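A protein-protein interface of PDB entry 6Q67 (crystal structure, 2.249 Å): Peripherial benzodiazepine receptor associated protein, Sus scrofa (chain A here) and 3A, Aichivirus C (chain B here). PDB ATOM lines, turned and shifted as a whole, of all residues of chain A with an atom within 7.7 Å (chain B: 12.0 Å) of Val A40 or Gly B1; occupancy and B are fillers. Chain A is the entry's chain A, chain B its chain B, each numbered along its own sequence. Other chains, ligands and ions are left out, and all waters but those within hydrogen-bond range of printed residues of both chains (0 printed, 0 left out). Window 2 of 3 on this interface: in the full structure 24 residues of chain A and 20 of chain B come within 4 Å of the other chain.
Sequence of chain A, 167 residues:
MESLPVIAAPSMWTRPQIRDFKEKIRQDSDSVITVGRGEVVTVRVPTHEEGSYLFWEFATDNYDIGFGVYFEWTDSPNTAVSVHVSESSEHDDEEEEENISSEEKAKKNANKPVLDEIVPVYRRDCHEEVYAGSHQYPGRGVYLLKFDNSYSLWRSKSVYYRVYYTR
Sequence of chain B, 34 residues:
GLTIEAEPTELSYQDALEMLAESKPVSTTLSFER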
ATOM      1  N   VAL A  35     -21.433 -18.323   9.415  1.00  0.00           N
ATOM      2  CA  VAL A  35     -20.213 -18.072   8.667  1.00  0.00           C
ATOM      3  C   VAL A  35     -20.516 -17.045   7.586  1.00  0.00           C
ATOM      4  O   VAL A  35     -21.329 -17.296   6.697  1.00  0.00           O
ATOM      5  CB  VAL A  35     -19.642 -19.352   8.029  1.00  0.00           C
ATOM      6  CG1 VAL A  35     -18.317 -19.045   7.321  1.00  0.00           C
ATOM      7  CG2 VAL A  35     -19.436 -20.425   9.081  1.00  0.00           C
ATOM      8  N   GLY A  36     -19.868 -15.888   7.672  1.00  0.00           N
ATOM      9  CA  GLY A  36     -20.101 -14.815   6.724  1.00  0.00           C
ATOM     10  C   GLY A  36     -19.715 -15.189   5.312  1.00  0.00           C
ATOM     11  O   GLY A  36     -18.957 -16.133   5.091  1.00  0.00           O
ATOM     12  N   ARG A  37     -20.245 -14.448   4.346  1.00  0.00           N
ATOM     13  CA  ARG A  37     -19.867 -14.648   2.959  1.00  0.00           C
ATOM     14  C   ARG A  37     -18.380 -14.365   2.832  1.00  0.00           C
ATOM     15  O   ARG A  37     -17.871 -13.423   3.434  1.00  0.00           O
ATOM     16  CB  ARG A  37     -20.685 -13.754   2.028  1.00  0.00           C
ATOM     17  CG  ARG A  37     -20.678 -12.285   2.409  1.00  0.00           C
ATOM     18  CD  ARG A  37     -21.708 -11.500   1.612  1.00  0.00           C
ATOM     19  NE  ARG A  37     -21.726 -10.088   1.981  1.00  0.00           N
ATOM     20  CZ  ARG A  37     -20.880  -9.175   1.511  1.00  0.00           C
ATOM     21  NH1 ARG A  37     -19.926  -9.514   0.651  1.00  0.00           N
ATOM     22  NH2 ARG A  37     -20.987  -7.915   1.909  1.00  0.00           N
ATOM     23  N   GLY A  38     -17.687 -15.229   2.098  1.00  0.00           N
ATOM     24  CA  GLY A  38     -16.253 -15.112   1.894  1.00  0.00           C
ATOM     25  C   GLY A  38     -15.350 -15.331   3.101  1.00  0.00           C
ATOM     26  O   GLY A  38     -14.150 -15.036   3.045  1.00  0.00           O
ATOM     27  N   GLU A  39     -15.901 -15.881   4.175  1.00  0.00           N
ATOM     28  CA  GLU A  39     -15.173 -15.991   5.434  1.00  0.00           C
ATOM     29  C   GLU A  39     -14.976 -17.428   5.889  1.00  0.00           C
ATOM     30  O   GLU A  39     -15.642 -18.366   5.420  1.00  0.00           O
ATOM     31  CB  GLU A  39     -15.889 -15.200   6.536  1.00  0.00           C
ATOM     32  CG  GLU A  39     -15.520 -13.713   6.550  1.00  0.00           C
ATOM     33  CD  GLU A  39     -16.175 -12.941   7.684  1.00  0.00           C
ATOM     34  OE1 GLU A  39     -17.022 -13.518   8.400  1.00  0.00           O
ATOM     35  OE2 GLU A  39     -15.834 -11.750   7.861  1.00  0.00           O
ATOM     36  N   VAL A  40     -14.025 -17.579   6.802  1.00  0.00           N
ATOM     37  CA  VAL A  40     -13.654 -18.871   7.344  1.00  0.00           C
ATOM     38  C   VAL A  40     -13.623 -18.835   8.851  1.00  0.00           C
ATOM     39  O   VAL A  40     -12.878 -18.052   9.434  1.00  0.00           O
ATOM     40  CB  VAL A  40     -12.280 -19.308   6.865  1.00  0.00           C
ATOM     41  CG1 VAL A  40     -12.010 -20.723   7.338  1.00  0.00           C
ATOM     42  CG2 VAL A  40     -12.196 -19.214   5.357  1.00  0.00           C
ATOM     43  N   VAL A  41     -14.422 -19.698   9.477  1.00  0.00           N
ATOM     44  CA  VAL A  41     -14.463 -19.783  10.923  1.00  0.00           C
ATOM     45  C   VAL A  41     -13.684 -21.016  11.373  1.00  0.00           C
ATOM     46  O   VAL A  41     -13.939 -22.122  10.897  1.00  0.00           O
ATOM     47  CB  VAL A  41     -15.909 -19.861  11.439  1.00  0.00           C
ATOM     48  CG1 VAL A  41     -15.934 -19.951  12.938  1.00  0.00           C
ATOM     49  CG2 VAL A  41     -16.694 -18.643  10.998  1.00  0.00           C
ATOM     50  N   THR A  42     -12.738 -20.823  12.286  1.00  0.00           N
ATOM     51  CA  THR A  42     -11.949 -21.928  12.810  1.00  0.00           C
ATOM     52  C   THR A  42     -12.411 -22.225  14.238  1.00  0.00           C
ATOM     53  O   THR A  42     -12.436 -21.334  15.087  1.00  0.00           O
ATOM     54  CB  THR A  42     -10.433 -21.611  12.758  1.00  0.00           C
ATOM     55  OG1 THR A  42     -10.039 -21.409  11.395  1.00  0.00           O
ATOM     56  CG2 THR A  42      -9.604 -22.750  13.315  1.00  0.00           C
ATOM     57  N   VAL A  43     -12.824 -23.468  14.479  1.00  0.00           N
ATOM     58  CA  VAL A  43     -13.210 -23.913  15.820  1.00  0.00           C
ATOM     59  C   VAL A  43     -12.043 -24.677  16.440  1.00  0.00           C
ATOM     60  O   VAL A  43     -11.620 -25.709  15.913  1.00  0.00           O
ATOM     61  CB  VAL A  43     -14.469 -24.804  15.792  1.00  0.00           C
ATOM     62  CG1 VAL A  43     -14.821 -25.289  17.193  1.00  0.00           C
ATOM     63  CG2 VAL A  43     -15.649 -24.053  15.200  1.00  0.00           C
ATOM     64  N   ILE A  65     -20.961 -26.240   2.561  1.00  0.00           N
ATOM     65  CA  ILE A  65     -19.861 -25.472   3.114  1.00  0.00           C
ATOM     66  C   ILE A  65     -18.629 -26.347   3.049  1.00  0.00           C
ATOM     67  O   ILE A  65     -18.737 -27.580   3.078  1.00  0.00           O
ATOM     68  CB  ILE A  65     -20.121 -25.042   4.560  1.00  0.00           C
ATOM     69  CG1 ILE A  65     -19.143 -23.934   4.972  1.00  0.00           C
ATOM     70  CG2 ILE A  65     -20.042 -26.263   5.490  1.00  0.00           C
ATOM     71  CD1 ILE A  65     -19.475 -23.326   6.334  1.00  0.00           C
ATOM     72  N   GLY A  66     -17.462 -25.718   2.954  1.00  0.00           N
ATOM     73  CA  GLY A  66     -16.217 -26.449   3.023  1.00  0.00           C
ATOM     74  C   GLY A  66     -15.950 -26.854   4.456  1.00  0.00           C
ATOM     75  O   GLY A  66     -16.122 -26.040   5.362  1.00  0.00           O
ATOM     76  N   VAL A 121      -9.769 -29.951   3.582  1.00  0.00           N
ATOM     77  CA  VAL A 121     -10.903 -29.068   3.369  1.00  0.00           C
ATOM     78  C   VAL A 121     -11.513 -29.361   1.997  1.00  0.00           C
ATOM     79  O   VAL A 121     -10.835 -29.327   0.972  1.00  0.00           O
ATOM     80  CB  VAL A 121     -10.495 -27.597   3.487  1.00  0.00           C
ATOM     81  CG1 VAL A 121     -11.661 -26.686   3.166  1.00  0.00           C
ATOM     82  CG2 VAL A 121      -9.982 -27.314   4.885  1.00  0.00           C
ATOM     83  N   LEU A 145     -11.095 -27.213  13.540  1.00  0.00           N
ATOM     84  CA  LEU A 145     -12.189 -27.450  12.610  1.00  0.00           C
ATOM     85  C   LEU A 145     -12.348 -26.220  11.743  1.00  0.00           C
ATOM     86  O   LEU A 145     -12.562 -25.119  12.244  1.00  0.00           O
ATOM     87  CB  LEU A 145     -13.492 -27.770  13.356  1.00  0.00           C
ATOM     88  CG  LEU A 145     -13.714 -29.251  13.708  1.00  0.00           C
ATOM     89  CD1 LEU A 145     -12.566 -29.819  14.507  1.00  0.00           C
ATOM     90  CD2 LEU A 145     -15.001 -29.462  14.491  1.00  0.00           C
ATOM     91  N   LYS A 146     -12.206 -26.413  10.437  1.00  0.00           N
ATOM     92  CA  LYS A 146     -12.304 -25.323   9.490  1.00  0.00           C
ATOM     93  C   LYS A 146     -13.637 -25.391   8.806  1.00  0.00           C
ATOM     94  O   LYS A 146     -13.879 -26.299   8.015  1.00  0.00           O
ATOM     95  CB  LYS A 146     -11.187 -25.379   8.432  1.00  0.00           C
ATOM     96  CG  LYS A 146      -9.776 -25.195   8.965  1.00  0.00           C
ATOM     97  CD  LYS A 146      -9.527 -23.773   9.418  1.00  0.00           C
ATOM     98  CE  LYS A 146      -8.055 -23.547   9.680  1.00  0.00           C
ATOM     99  NZ  LYS A 146      -7.812 -22.198  10.243  1.00  0.00           N
ATOM    100  N   PHE A 147     -14.489 -24.416   9.096  1.00  0.00           N
ATOM    101  CA  PHE A 147     -15.704 -24.231   8.327  1.00  0.00           C
ATOM    102  C   PHE A 147     -15.425 -23.106   7.342  1.00  0.00           C
ATOM    103  O   PHE A 147     -15.312 -21.940   7.719  1.00  0.00           O
ATOM    104  CB  PHE A 147     -16.885 -23.899   9.218  1.00  0.00           C
ATOM    105  CG  PHE A 147     -17.256 -25.008  10.187  1.00  0.00           C
ATOM    106  CD1 PHE A 147     -17.895 -26.144   9.744  1.00  0.00           C
ATOM    107  CD2 PHE A 147     -16.972 -24.894  11.534  1.00  0.00           C
ATOM    108  CE1 PHE A 147     -18.247 -27.148  10.628  1.00  0.00           C
ATOM    109  CE2 PHE A 147     -17.318 -25.893  12.426  1.00  0.00           C
ATOM    110  CZ  PHE A 147     -17.954 -27.019  11.973  1.00  0.00           C
ATOM    111  N   ASP A 148     -15.330 -23.484   6.074  1.00  0.00           N
ATOM    112  CA  ASP A 148     -14.756 -22.639   5.052  1.00  0.00           C
ATOM    113  C   ASP A 148     -15.772 -22.194   4.007  1.00  0.00           C
ATOM    114  O   ASP A 148     -16.138 -22.970   3.129  1.00  0.00           O
ATOM    115  CB  ASP A 148     -13.624 -23.410   4.379  1.00  0.00           C
ATOM    116  CG  ASP A 148     -12.722 -22.524   3.532  1.00  0.00           C
ATOM    117  OD1 ASP A 148     -13.242 -21.588   2.894  1.00  0.00           O
ATOM    118  OD2 ASP A 148     -11.494 -22.777   3.500  1.00  0.00           O
ATOM    119  N   ASN A 149     -16.188 -20.930   4.098  1.00  0.00           N
ATOM    120  CA  ASN A 149     -17.145 -20.308   3.178  1.00  0.00           C
ATOM    121  C   ASN A 149     -16.492 -19.358   2.144  1.00  0.00           C
ATOM    122  O   ASN A 149     -17.173 -18.579   1.469  1.00  0.00           O
ATOM    123  CB  ASN A 149     -18.213 -19.562   3.976  1.00  0.00           C
ATOM    124  CG  ASN A 149     -19.502 -19.366   3.196  1.00  0.00           C
ATOM    125  OD1 ASN A 149     -19.838 -20.144   2.300  1.00  0.00           O
ATOM    126  ND2 ASN A 149     -20.235 -18.316   3.541  1.00  0.00           N
ATOM    127  N   SER A 150     -15.172 -19.366   2.086  1.00  0.00           N
ATOM    128  CA  SER A 150     -14.417 -18.369   1.310  1.00  0.00           C
ATOM    129  C   SER A 150     -14.756 -18.279  -0.190  1.00  0.00           C
ATOM    130  O   SER A 150     -14.460 -17.272  -0.829  1.00  0.00           O
ATOM    131  CB  SER A 150     -12.927 -18.652   1.464  1.00  0.00           C
ATOM    132  OG  SER A 150     -12.552 -19.774   0.693  1.00  0.00           O
ATOM    133  N   TYR A 151     -15.355 -19.328  -0.748  1.00  0.00           N
ATOM    134  CA  TYR A 151     -15.726 -19.360  -2.172  1.00  0.00           C
ATOM    135  C   TYR A 151     -17.112 -18.783  -2.431  1.00  0.00           C
ATOM    136  O   TYR A 151     -17.555 -18.702  -3.575  1.00  0.00           O
ATOM    137  CB  TYR A 151     -15.696 -20.794  -2.694  1.00  0.00           C
ATOM    138  CG  TYR A 151     -16.693 -21.698  -1.971  1.00  0.00           C
ATOM    139  CD1 TYR A 151     -16.349 -22.336  -0.784  1.00  0.00           C
ATOM    140  CD2 TYR A 151     -17.971 -21.900  -2.469  1.00  0.00           C
ATOM    141  CE1 TYR A 151     -17.245 -23.157  -0.112  1.00  0.00           C
ATOM    142  CE2 TYR A 151     -18.882 -22.720  -1.799  1.00  0.00           C
ATOM    143  CZ  TYR A 151     -18.507 -23.347  -0.619  1.00  0.00           C
ATOM    144  OH  TYR A 151     -19.388 -24.159   0.063  1.00  0.00           O
ATOM    145  N   GLY B   1     -11.774 -14.820   9.186  1.00  0.00           N
ATOM    146  CA  GLY B   1     -10.637 -14.937  10.147  1.00  0.00           C
ATOM    147  C   GLY B   1     -11.060 -15.199  11.589  1.00  0.00           C
ATOM    148  O   GLY B   1     -10.205 -15.276  12.475  1.00  0.00           O
ATOM    149  N   LEU B   2     -12.363 -15.339  11.836  1.00  0.00           N
ATOM    150  CA  LEU B   2     -12.859 -15.561  13.198  1.00  0.00           C
ATOM    151  C   LEU B   2     -12.413 -16.915  13.763  1.00  0.00           C
ATOM    152  O   LEU B   2     -12.309 -17.903  13.032  1.00  0.00           O
ATOM    153  CB  LEU B   2     -14.389 -15.469  13.243  1.00  0.00           C
ATOM    154  CG  LEU B   2     -15.030 -15.701  14.623  1.00  0.00           C
ATOM    155  CD1 LEU B   2     -14.617 -14.618  15.611  1.00  0.00           C
ATOM    156  CD2 LEU B   2     -16.560 -15.802  14.537  1.00  0.00           C
ATOM    157  N   THR B   3     -12.166 -16.942  15.075  1.00  0.00           N
ATOM    158  CA  THR B   3     -11.677 -18.134  15.767  1.00  0.00           C
ATOM    159  C   THR B   3     -12.443 -18.369  17.073  1.00  0.00           C
ATOM    160  O   THR B   3     -12.417 -17.530  17.971  1.00  0.00           O
ATOM    161  CB  THR B   3     -10.163 -18.020  16.072  1.00  0.00           C
ATOM    162  OG1 THR B   3      -9.433 -17.883  14.846  1.00  0.00           O
ATOM    163  CG2 THR B   3      -9.655 -19.254  16.815  1.00  0.00           C
ATOM    164  N   ILE B   4     -13.106 -19.524  17.160  1.00  0.00           N
ATOM    165  CA  ILE B   4     -13.916 -19.919  18.319  1.00  0.00           C
ATOM    166  C   ILE B   4     -13.228 -21.006  19.134  1.00  0.00           C
ATOM    167  O   ILE B   4     -12.552 -21.864  18.567  1.00  0.00           O
ATOM    168  CB  ILE B   4     -15.290 -20.459  17.876  1.00  0.00           C
ATOM    169  CG1 ILE B   4     -16.028 -19.431  17.022  1.00  0.00           C
ATOM    170  CG2 ILE B   4     -16.144 -20.861  19.077  1.00  0.00           C
ATOM    171  CD1 ILE B   4     -16.240 -18.111  17.716  1.00  0.00           C
ATOM    172  N   GLU B   5     -13.418 -20.989  20.453  1.00  0.00           N
ATOM    173  CA  GLU B   5     -12.852 -22.026  21.306  1.00  0.00           C
ATOM    174  C   GLU B   5     -13.962 -22.845  21.960  1.00  0.00           C
ATOM    175  O   GLU B   5     -14.770 -22.333  22.740  1.00  0.00           O
ATOM    176  CB  GLU B   5     -11.919 -21.406  22.348  1.00  0.00           C
ATOM    177  CG  GLU B   5     -10.615 -20.898  21.721  1.00  0.00           C
ATOM    178  CD  GLU B   5      -9.702 -20.213  22.711  1.00  0.00           C
ATOM    179  OE1 GLU B   5      -9.965 -20.311  23.929  1.00  0.00           O
ATOM    180  OE2 GLU B   5      -8.719 -19.576  22.269  1.00  0.00           O
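O of Val A40 is in hydrogen-bond range of N of Gly B1 (3.4 Å).
The backbone NH (N) of Thr A42 sits at hydrogen-bond distance from the backbone carbonyl oxygen (O) of Leu B2, at 3.0 Å.
The backbone NH (N) of Ile B4 sits at hydrogen-bond distance from the backbone carbonyl oxygen (O) of Thr A42, 2.8 Å away.
N of Phe A147 is in hydrogen-bond range of O of Val A41.
The side-chain amino group (NZ) of Lys A146 is in hydrogen-bond range of the side-chain hydroxyl (OG1) of Thr A42 (2.6 Å).
The backbone NH (N) of Val A43 is in hydrogen-bond range of the backbone carbonyl oxygen (O) of Leu A145 (2.8 Å).
Among the printed residues, pairs that only touch across the chains: Thr A42 with Thr B3, Val A43 with Ile B4, Val A41 with Leu B2 and Val A40 with Leu B2.
Val A40 touches just these residues of chain B: Gly B1 and Leu B2.
Of chain A, only Val A40 (3.4 Å) comes within 4 Å of Gly B1.
No residue of chain B comes within 4 Å of Gly A36.
No residue of chain B comes within 4 Å of Gly A38.
No residue of chain B comes within 4 Å of Glu A39.
Of the printed residues of chain B, Val A41 touches Leu B2 (3.6 Å).
Thr A42 touches three residues of chain B.
No residue of chain B comes within 4 Å of Asp A148.
No residue of chain B comes within 4 Å of Asn A149.
No residue of chain B comes within 4 Å of Ser A150.
Of the printed residues of chain A, Leu B2 touches Val A40, Val A41 and Thr A42.
Of the printed residues of chain B, Val A43 touches Ile B4 (3.5 Å).
Printed residues of chain A within 4 Å of Ile B4: Thr A42 and Val A43.
Printed residues of chain A within 4 Å of Thr B3: Thr A42.
The nearest residue of chain B that does not touch Val A40 is Thr B3 (5.8 Å).
The nearest printed residue of chain A that does not touch Ile B4 is Val A41 (4.1 Å).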
